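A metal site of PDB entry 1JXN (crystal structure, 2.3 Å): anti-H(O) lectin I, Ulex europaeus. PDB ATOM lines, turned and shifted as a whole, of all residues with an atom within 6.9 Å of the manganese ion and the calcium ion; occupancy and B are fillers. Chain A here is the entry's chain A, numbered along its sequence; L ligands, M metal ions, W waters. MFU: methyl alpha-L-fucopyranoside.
NE1 of Trp 136 sits close to OD1 of Asp 137.
The backbone carbonyl oxygen (O) of Asp 137 sits close to the backbone NH (N) of Ser 131, 3.5 Å away.
NE2 of His 142 lies close to OE1 of Glu 125, at 3.1 Å.
The backbone NH of Glu 125 lies within hydrogen-bond range of the backbone carbonyl oxygen of Gly 144, at 2.7 Å.
O of His 142 sits at hydrogen-bond distance from N of Asp 127 (2.7 Å).
Of the 24 residues printed, 4 come within 4 Å of the manganese ion.
The nearest printed residue that does not touch the manganese ion is Val 150 (4.2 Å).
The manganese ion is bound by water W3 (2.2 Å), water W1 (2.2 Å), OE1 of Glu 125 (2.2 Å), OD1 of Asp 127 (2.3 Å) and OD2 of Asp 137 (2.4 Å).
The manganese ion has five donor atoms within binding distance.
Slightly farther from the manganese ion lies a ring nitrogen (NE2) of His 142 (2.7 Å).
Water W3 lies within hydrogen-bond range of OG of Ser 152 and NE2 of His 142.
Water W1 lies within hydrogen-bond range of the backbone carbonyl oxygen of Val 150, the side-chain carboxylate of Glu 125 and the indole nitrogen of Trp 136.
Water W4 lies within hydrogen-bond range of the backbone carbonyl oxygen (O) of Gly 105 (2.6 Å) and the indole nitrogen (NE1) of Trp 136 (2.8 Å).
An oxygen (O4) of the ligand sits at hydrogen-bond distance from the side-chain amide nitrogen (ND2) of Asn 134 (2.9 Å).
An oxygen (O4) of the ligand is in hydrogen-bond range of the backbone NH of Gly 105 (2.8 Å).
An oxygen (O4) of the ligand sits at hydrogen-bond distance from the side-chain carboxylate (OD2) of Asp 87, 2.7 Å away.
Water W2 binds the calcium ion (2.2 Å).
OD1 of Asp 127 is bound to the calcium ion (2.2 Å).
OD1 of Asp 137 binds the calcium ion (2.3 Å).
The side-chain carboxylate (OD2) of Asp 127 binds the calcium ion, 2.3 Å away.
Water W4 binds the calcium ion (2.4 Å).
OD1 of Asn 134 binds the calcium ion, at 2.4 Å.
The calcium ion is bound by O of Ile 129 (2.5 Å).
Of the 24 residues printed, 4 come within 4 Å of the calcium ion.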
ATOM      1  N   ASP A  87      14.645   8.964   9.252  1.00  0.00           N
ATOM      2  CA  ASP A  87      13.542   9.678   8.586  1.00  0.00           C
ATOM      3  C   ASP A  87      12.816   8.623   7.778  1.00  0.00           C
ATOM      4  O   ASP A  87      11.673   8.831   7.373  1.00  0.00           O
ATOM      5  CB  ASP A  87      14.075  10.685   7.604  1.00  0.00           C
ATOM      6  CG  ASP A  87      14.421  11.977   8.243  1.00  0.00           C
ATOM      7  OD1 ASP A  87      15.602  12.163   8.611  1.00  0.00           O
ATOM      8  OD2 ASP A  87      13.507  12.825   8.386  1.00  0.00           O
ATOM      9  N   GLY A 104      17.767  13.343   4.928  1.00  0.00           N
ATOM     10  CA  GLY A 104      16.921  13.686   6.053  1.00  0.00           C
ATOM     11  C   GLY A 104      15.480  13.418   5.663  1.00  0.00           C
ATOM     12  O   GLY A 104      15.161  12.324   5.184  1.00  0.00           O
ATOM     13  N   GLY A 105      14.624  14.412   5.848  1.00  0.00           N
ATOM     14  CA  GLY A 105      13.220  14.244   5.521  1.00  0.00           C
ATOM     15  C   GLY A 105      12.927  14.195   4.042  1.00  0.00           C
ATOM     16  O   GLY A 105      11.829  13.833   3.630  1.00  0.00           O
ATOM     17  N   TYR A 106      13.907  14.565   3.234  1.00  0.00           N
ATOM     18  CA  TYR A 106      13.737  14.577   1.794  1.00  0.00           C
ATOM     19  C   TYR A 106      14.162  13.284   1.130  1.00  0.00           C
ATOM     20  O   TYR A 106      14.011  13.129  -0.082  1.00  0.00           O
ATOM     21  CB  TYR A 106      14.450  15.778   1.209  1.00  0.00           C
ATOM     22  CG  TYR A 106      13.848  17.071   1.706  1.00  0.00           C
ATOM     23  CD1 TYR A 106      14.330  17.689   2.881  1.00  0.00           C
ATOM     24  CD2 TYR A 106      12.788  17.679   1.029  1.00  0.00           C
ATOM     25  CE1 TYR A 106      13.755  18.872   3.350  1.00  0.00           C
ATOM     26  CE2 TYR A 106      12.215  18.849   1.493  1.00  0.00           C
ATOM     27  CZ  TYR A 106      12.710  19.443   2.652  1.00  0.00           C
ATOM     28  OH  TYR A 106      12.170  20.623   3.055  1.00  0.00           O
ATOM     29  N   PHE A 107      14.691  12.353   1.926  1.00  0.00           N
ATOM     30  CA  PHE A 107      15.109  11.025   1.477  1.00  0.00           C
ATOM     31  C   PHE A 107      16.204  10.885   0.411  1.00  0.00           C
ATOM     32  O   PHE A 107      16.564   9.766   0.041  1.00  0.00           O
ATOM     33  CB  PHE A 107      13.878  10.248   1.005  1.00  0.00           C
ATOM     34  CG  PHE A 107      12.829  10.077   2.058  1.00  0.00           C
ATOM     35  CD1 PHE A 107      11.619  10.760   1.969  1.00  0.00           C
ATOM     36  CD2 PHE A 107      13.043   9.206   3.134  1.00  0.00           C
ATOM     37  CE1 PHE A 107      10.632  10.589   2.931  1.00  0.00           C
ATOM     38  CE2 PHE A 107      12.065   9.029   4.113  1.00  0.00           C
ATOM     39  CZ  PHE A 107      10.861   9.721   4.023  1.00  0.00           C
ATOM     40  N   GLU A 125       7.199   5.911  -0.099  1.00  0.00           N
ATOM     41  CA  GLU A 125       7.928   6.172   1.119  1.00  0.00           C
ATOM     42  C   GLU A 125       7.389   5.482   2.366  1.00  0.00           C
ATOM     43  O   GLU A 125       6.227   5.102   2.441  1.00  0.00           O
ATOM     44  CB  GLU A 125       8.015   7.677   1.389  1.00  0.00           C
ATOM     45  CG  GLU A 125       6.669   8.339   1.621  1.00  0.00           C
ATOM     46  CD  GLU A 125       6.768   9.657   2.339  1.00  0.00           C
ATOM     47  OE1 GLU A 125       6.200   9.767   3.440  1.00  0.00           O
ATOM     48  OE2 GLU A 125       7.400  10.597   1.814  1.00  0.00           O
ATOM     49  N   PHE A 126       8.303   5.268   3.301  1.00  0.00           N
ATOM     50  CA  PHE A 126       8.036   4.665   4.601  1.00  0.00           C
ATOM     51  C   PHE A 126       8.688   5.704   5.500  1.00  0.00           C
ATOM     52  O   PHE A 126       9.876   5.610   5.851  1.00  0.00           O
ATOM     53  CB  PHE A 126       8.734   3.316   4.718  1.00  0.00           C
ATOM     54  CG  PHE A 126       8.324   2.339   3.666  1.00  0.00           C
ATOM     55  CD1 PHE A 126       8.789   2.483   2.353  1.00  0.00           C
ATOM     56  CD2 PHE A 126       7.423   1.325   3.941  1.00  0.00           C
ATOM     57  CE1 PHE A 126       8.366   1.630   1.351  1.00  0.00           C
ATOM     58  CE2 PHE A 126       6.987   0.470   2.945  1.00  0.00           C
ATOM     59  CZ  PHE A 126       7.462   0.632   1.645  1.00  0.00           C
ATOM     60  N   ASP A 127       7.917   6.751   5.778  1.00  0.00           N
ATOM     61  CA  ASP A 127       8.331   7.900   6.569  1.00  0.00           C
ATOM     62  C   ASP A 127       8.208   7.660   8.071  1.00  0.00           C
ATOM     63  O   ASP A 127       7.110   7.427   8.575  1.00  0.00           O
ATOM     64  CB  ASP A 127       7.458   9.092   6.159  1.00  0.00           C
ATOM     65  CG  ASP A 127       8.055  10.410   6.523  1.00  0.00           C
ATOM     66  OD1 ASP A 127       7.829  11.379   5.771  1.00  0.00           O
ATOM     67  OD2 ASP A 127       8.764  10.502   7.540  1.00  0.00           O
ATOM     68  N   THR A 128       9.317   7.741   8.793  1.00  0.00           N
ATOM     69  CA  THR A 128       9.286   7.505  10.237  1.00  0.00           C
ATOM     70  C   THR A 128       9.099   8.744  11.124  1.00  0.00           C
ATOM     71  O   THR A 128       8.881   8.597  12.319  1.00  0.00           O
ATOM     72  CB  THR A 128      10.526   6.729  10.703  1.00  0.00           C
ATOM     73  OG1 THR A 128      11.702   7.514  10.454  1.00  0.00           O
ATOM     74  CG2 THR A 128      10.659   5.400   9.968  1.00  0.00           C
ATOM     75  N   ILE A 129       9.225   9.946  10.551  1.00  0.00           N
ATOM     76  CA  ILE A 129       9.017  11.171  11.349  1.00  0.00           C
ATOM     77  C   ILE A 129       8.250  12.267  10.581  1.00  0.00           C
ATOM     78  O   ILE A 129       8.721  12.806   9.565  1.00  0.00           O
ATOM     79  CB  ILE A 129      10.338  11.725  11.947  1.00  0.00           C
ATOM     80  CG1 ILE A 129      10.044  12.488  13.245  1.00  0.00           C
ATOM     81  CG2 ILE A 129      11.067  12.634  10.971  1.00  0.00           C
ATOM     82  CD1 ILE A 129       9.604  11.620  14.415  1.00  0.00           C
ATOM     83  N   GLY A 130       7.042  12.563  11.065  1.00  0.00           N
ATOM     84  CA  GLY A 130       6.202  13.558  10.417  1.00  0.00           C
ATOM     85  C   GLY A 130       6.104  14.850  11.194  1.00  0.00           C
ATOM     86  O   GLY A 130       7.013  15.194  11.969  1.00  0.00           O
ATOM     87  N   SER A 131       5.018  15.596  10.954  1.00  0.00           N
ATOM     88  CA  SER A 131       4.744  16.878  11.631  1.00  0.00           C
ATOM     89  C   SER A 131       4.636  16.677  13.150  1.00  0.00           C
ATOM     90  O   SER A 131       4.109  15.655  13.605  1.00  0.00           O
ATOM     91  CB  SER A 131       3.436  17.477  11.103  1.00  0.00           C
ATOM     92  OG  SER A 131       3.522  18.895  11.061  1.00  0.00           O
ATOM     93  N   ASN A 134       8.608  17.408  10.764  1.00  0.00           N
ATOM     94  CA  ASN A 134       8.599  17.474   9.306  1.00  0.00           C
ATOM     95  C   ASN A 134       7.262  18.103   8.958  1.00  0.00           C
ATOM     96  O   ASN A 134       6.256  17.421   8.789  1.00  0.00           O
ATOM     97  CB  ASN A 134       8.693  16.067   8.693  1.00  0.00           C
ATOM     98  CG  ASN A 134      10.131  15.634   8.408  1.00  0.00           C
ATOM     99  OD1 ASN A 134      10.359  14.566   7.841  1.00  0.00           O
ATOM    100  ND2 ASN A 134      11.101  16.464   8.800  1.00  0.00           N
ATOM    101  N   TRP A 136       5.594  19.425   6.367  1.00  0.00           N
ATOM    102  CA  TRP A 136       4.836  18.914   5.209  1.00  0.00           C
ATOM    103  C   TRP A 136       4.169  17.546   5.335  1.00  0.00           C
ATOM    104  O   TRP A 136       3.472  17.112   4.406  1.00  0.00           O
ATOM    105  CB  TRP A 136       5.759  18.846   3.985  1.00  0.00           C
ATOM    106  CG  TRP A 136       6.957  17.967   4.215  1.00  0.00           C
ATOM    107  CD1 TRP A 136       7.049  16.615   3.963  1.00  0.00           C
ATOM    108  CD2 TRP A 136       8.220  18.349   4.759  1.00  0.00           C
ATOM    109  NE1 TRP A 136       8.293  16.155   4.312  1.00  0.00           N
ATOM    110  CE2 TRP A 136       9.038  17.194   4.798  1.00  0.00           C
ATOM    111  CE3 TRP A 136       8.750  19.571   5.208  1.00  0.00           C
ATOM    112  CZ2 TRP A 136      10.347  17.228   5.271  1.00  0.00           C
ATOM    113  CZ3 TRP A 136      10.059  19.591   5.676  1.00  0.00           C
ATOM    114  CH2 TRP A 136      10.844  18.424   5.704  1.00  0.00           C
ATOM    115  N   ASP A 137       4.412  16.866   6.449  1.00  0.00           N
ATOM    116  CA  ASP A 137       3.865  15.526   6.699  1.00  0.00           C
ATOM    117  C   ASP A 137       2.757  15.474   7.731  1.00  0.00           C
ATOM    118  O   ASP A 137       2.613  16.391   8.555  1.00  0.00           O
ATOM    119  CB  ASP A 137       4.935  14.621   7.305  1.00  0.00           C
ATOM    120  CG  ASP A 137       5.969  14.183   6.321  1.00  0.00           C
ATOM    121  OD1 ASP A 137       7.122  14.006   6.767  1.00  0.00           O
ATOM    122  OD2 ASP A 137       5.638  13.977   5.139  1.00  0.00           O
ATOM    123  N   PRO A 138       1.978  14.382   7.727  1.00  0.00           N
ATOM    124  CA  PRO A 138       0.907  14.224   8.702  1.00  0.00           C
ATOM    125  C   PRO A 138       1.572  14.103  10.082  1.00  0.00           C
ATOM    126  O   PRO A 138       2.801  13.981  10.190  1.00  0.00           O
ATOM    127  CB  PRO A 138       0.227  12.902   8.274  1.00  0.00           C
ATOM    128  CG  PRO A 138       1.215  12.240   7.379  1.00  0.00           C
ATOM    129  CD  PRO A 138       1.818  13.392   6.646  1.00  0.00           C
ATOM    130  N   HIS A 142       4.405   7.296   8.927  1.00  0.00           N
ATOM    131  CA  HIS A 142       3.479   6.768   7.932  1.00  0.00           C
ATOM    132  C   HIS A 142       4.157   6.269   6.653  1.00  0.00           C
ATOM    133  O   HIS A 142       5.393   6.316   6.509  1.00  0.00           O
ATOM    134  CB  HIS A 142       2.503   7.887   7.539  1.00  0.00           C
ATOM    135  CG  HIS A 142       3.179   9.065   6.930  1.00  0.00           C
ATOM    136  ND1 HIS A 142       4.130   9.821   7.578  1.00  0.00           N
ATOM    137  CD2 HIS A 142       3.117   9.553   5.668  1.00  0.00           C
ATOM    138  CE1 HIS A 142       4.630  10.707   6.713  1.00  0.00           C
ATOM    139  NE2 HIS A 142       4.046  10.589   5.539  1.00  0.00           N
ATOM    140  N   ILE A 143       3.301   5.816   5.730  1.00  0.00           N
ATOM    141  CA  ILE A 143       3.698   5.313   4.420  1.00  0.00           C
ATOM    142  C   ILE A 143       2.980   6.186   3.385  1.00  0.00           C
ATOM    143  O   ILE A 143       1.822   6.531   3.564  1.00  0.00           O
ATOM    144  CB  ILE A 143       3.282   3.846   4.300  1.00  0.00           C
ATOM    145  CG1 ILE A 143       4.231   2.991   5.138  1.00  0.00           C
ATOM    146  CG2 ILE A 143       3.236   3.390   2.836  1.00  0.00           C
ATOM    147  CD1 ILE A 143       3.794   1.565   5.291  1.00  0.00           C
ATOM    148  N   GLY A 144       3.668   6.574   2.322  1.00  0.00           N
ATOM    149  CA  GLY A 144       3.026   7.393   1.323  1.00  0.00           C
ATOM    150  C   GLY A 144       3.569   7.250  -0.082  1.00  0.00           C
ATOM    151  O   GLY A 144       4.637   6.671  -0.295  1.00  0.00           O
ATOM    152  N   ASP A 146       4.847   9.328  -3.183  1.00  0.00           N
ATOM    153  CA  ASP A 146       5.377  10.638  -3.541  1.00  0.00           C
ATOM    154  C   ASP A 146       5.454  10.825  -5.049  1.00  0.00           C
ATOM    155  O   ASP A 146       6.182  10.104  -5.723  1.00  0.00           O
ATOM    156  CB  ASP A 146       6.777  10.833  -2.979  1.00  0.00           C
ATOM    157  CG  ASP A 146       6.852  10.720  -1.465  1.00  0.00           C
ATOM    158  OD1 ASP A 146       5.853  10.357  -0.821  1.00  0.00           O
ATOM    159  OD2 ASP A 146       7.954  10.985  -0.935  1.00  0.00           O
ATOM    160  N   VAL A 150       8.056  15.818  -2.115  1.00  0.00           N
ATOM    161  CA  VAL A 150       8.287  15.181  -0.815  1.00  0.00           C
ATOM    162  C   VAL A 150       6.992  15.034  -0.002  1.00  0.00           C
ATOM    163  O   VAL A 150       6.950  14.299   0.994  1.00  0.00           O
ATOM    164  CB  VAL A 150       9.315  15.951   0.033  1.00  0.00           C
ATOM    165  CG1 VAL A 150       8.730  17.257   0.537  1.00  0.00           C
ATOM    166  CG2 VAL A 150       9.809  15.073   1.148  1.00  0.00           C
ATOM    167  N   LYS A 151       5.966  15.750  -0.459  1.00  0.00           N
ATOM    168  CA  LYS A 151       4.630  15.723   0.145  1.00  0.00           C
ATOM    169  C   LYS A 151       3.822  14.681  -0.627  1.00  0.00           C
ATOM    170  O   LYS A 151       3.662  14.807  -1.844  1.00  0.00           O
ATOM    171  CB  LYS A 151       3.983  17.106  -0.034  1.00  0.00           C
ATOM    172  CG  LYS A 151       3.007  17.519   1.064  1.00  0.00           C
ATOM    173  CD  LYS A 151       2.539  18.956   0.869  1.00  0.00           C
ATOM    174  CE  LYS A 151       3.716  19.948   0.796  1.00  0.00           C
ATOM    175  NZ  LYS A 151       4.483  19.917  -0.511  1.00  0.00           N
ATOM    176  N   SER A 152       3.314  13.655   0.064  1.00  0.00           N
ATOM    177  CA  SER A 152       2.537  12.596  -0.577  1.00  0.00           C
ATOM    178  C   SER A 152       1.193  12.992  -1.214  1.00  0.00           C
ATOM    179  O   SER A 152       0.614  14.049  -0.892  1.00  0.00           O
ATOM    180  CB  SER A 152       2.282  11.471   0.420  1.00  0.00           C
ATOM    181  OG  SER A 152       3.480  11.031   1.012  1.00  0.00           O
ATOM    182  N   ALA A 155      -1.487   9.051   1.874  1.00  0.00           N
ATOM    183  CA  ALA A 155      -0.640   8.405   2.885  1.00  0.00           C
ATOM    184  C   ALA A 155      -1.428   7.578   3.896  1.00  0.00           C
ATOM    185  O   ALA A 155      -2.664   7.612   3.904  1.00  0.00           O
ATOM    186  CB  ALA A 155       0.200   9.446   3.605  1.00  0.00           C
HETATM  187  C1  MFU L   1      14.085  18.733   9.589  1.00  0.00           C
HETATM  188  C2  MFU L   1      14.314  18.371   8.096  1.00  0.00           C
HETATM  189  C3  MFU L   1      15.432  17.301   8.054  1.00  0.00           C
HETATM  190  C4  MFU L   1      14.994  16.068   8.886  1.00  0.00           C
HETATM  191  C5  MFU L   1      14.732  16.490  10.334  1.00  0.00           C
HETATM  192  C6  MFU L   1      14.286  15.276  11.176  1.00  0.00           C
HETATM  193  O1  MFU L   1      15.317  19.350  10.125  1.00  0.00           O
HETATM  194  O2  MFU L   1      14.655  19.542   7.353  1.00  0.00           O
HETATM  195  O3  MFU L   1      15.683  16.930   6.712  1.00  0.00           O
HETATM  196  O4  MFU L   1      13.795  15.513   8.331  1.00  0.00           O
HETATM  197  O5  MFU L   1      13.737  17.531  10.372  1.00  0.00           O
HETATM  198  CM  MFU L   1      15.950  20.641   9.918  1.00  0.00           C
HETATM  199 MN    MN M   1       6.147  11.814   4.286  1.00  0.00          MN
HETATM  200 CA    CA M   2       9.015  12.787   7.060  1.00  0.00          CA
HETATM  201  O   HOH W   1       7.492  13.145   3.145  1.00  0.00           O
HETATM  202  O   HOH W   2      11.104  12.002   7.211  1.00  0.00           O
HETATM  203  O   HOH W   3       4.219  11.868   3.282  1.00  0.00           O
HETATM  204  O   HOH W   4       9.559  13.697   4.956  1.00  0.00           O
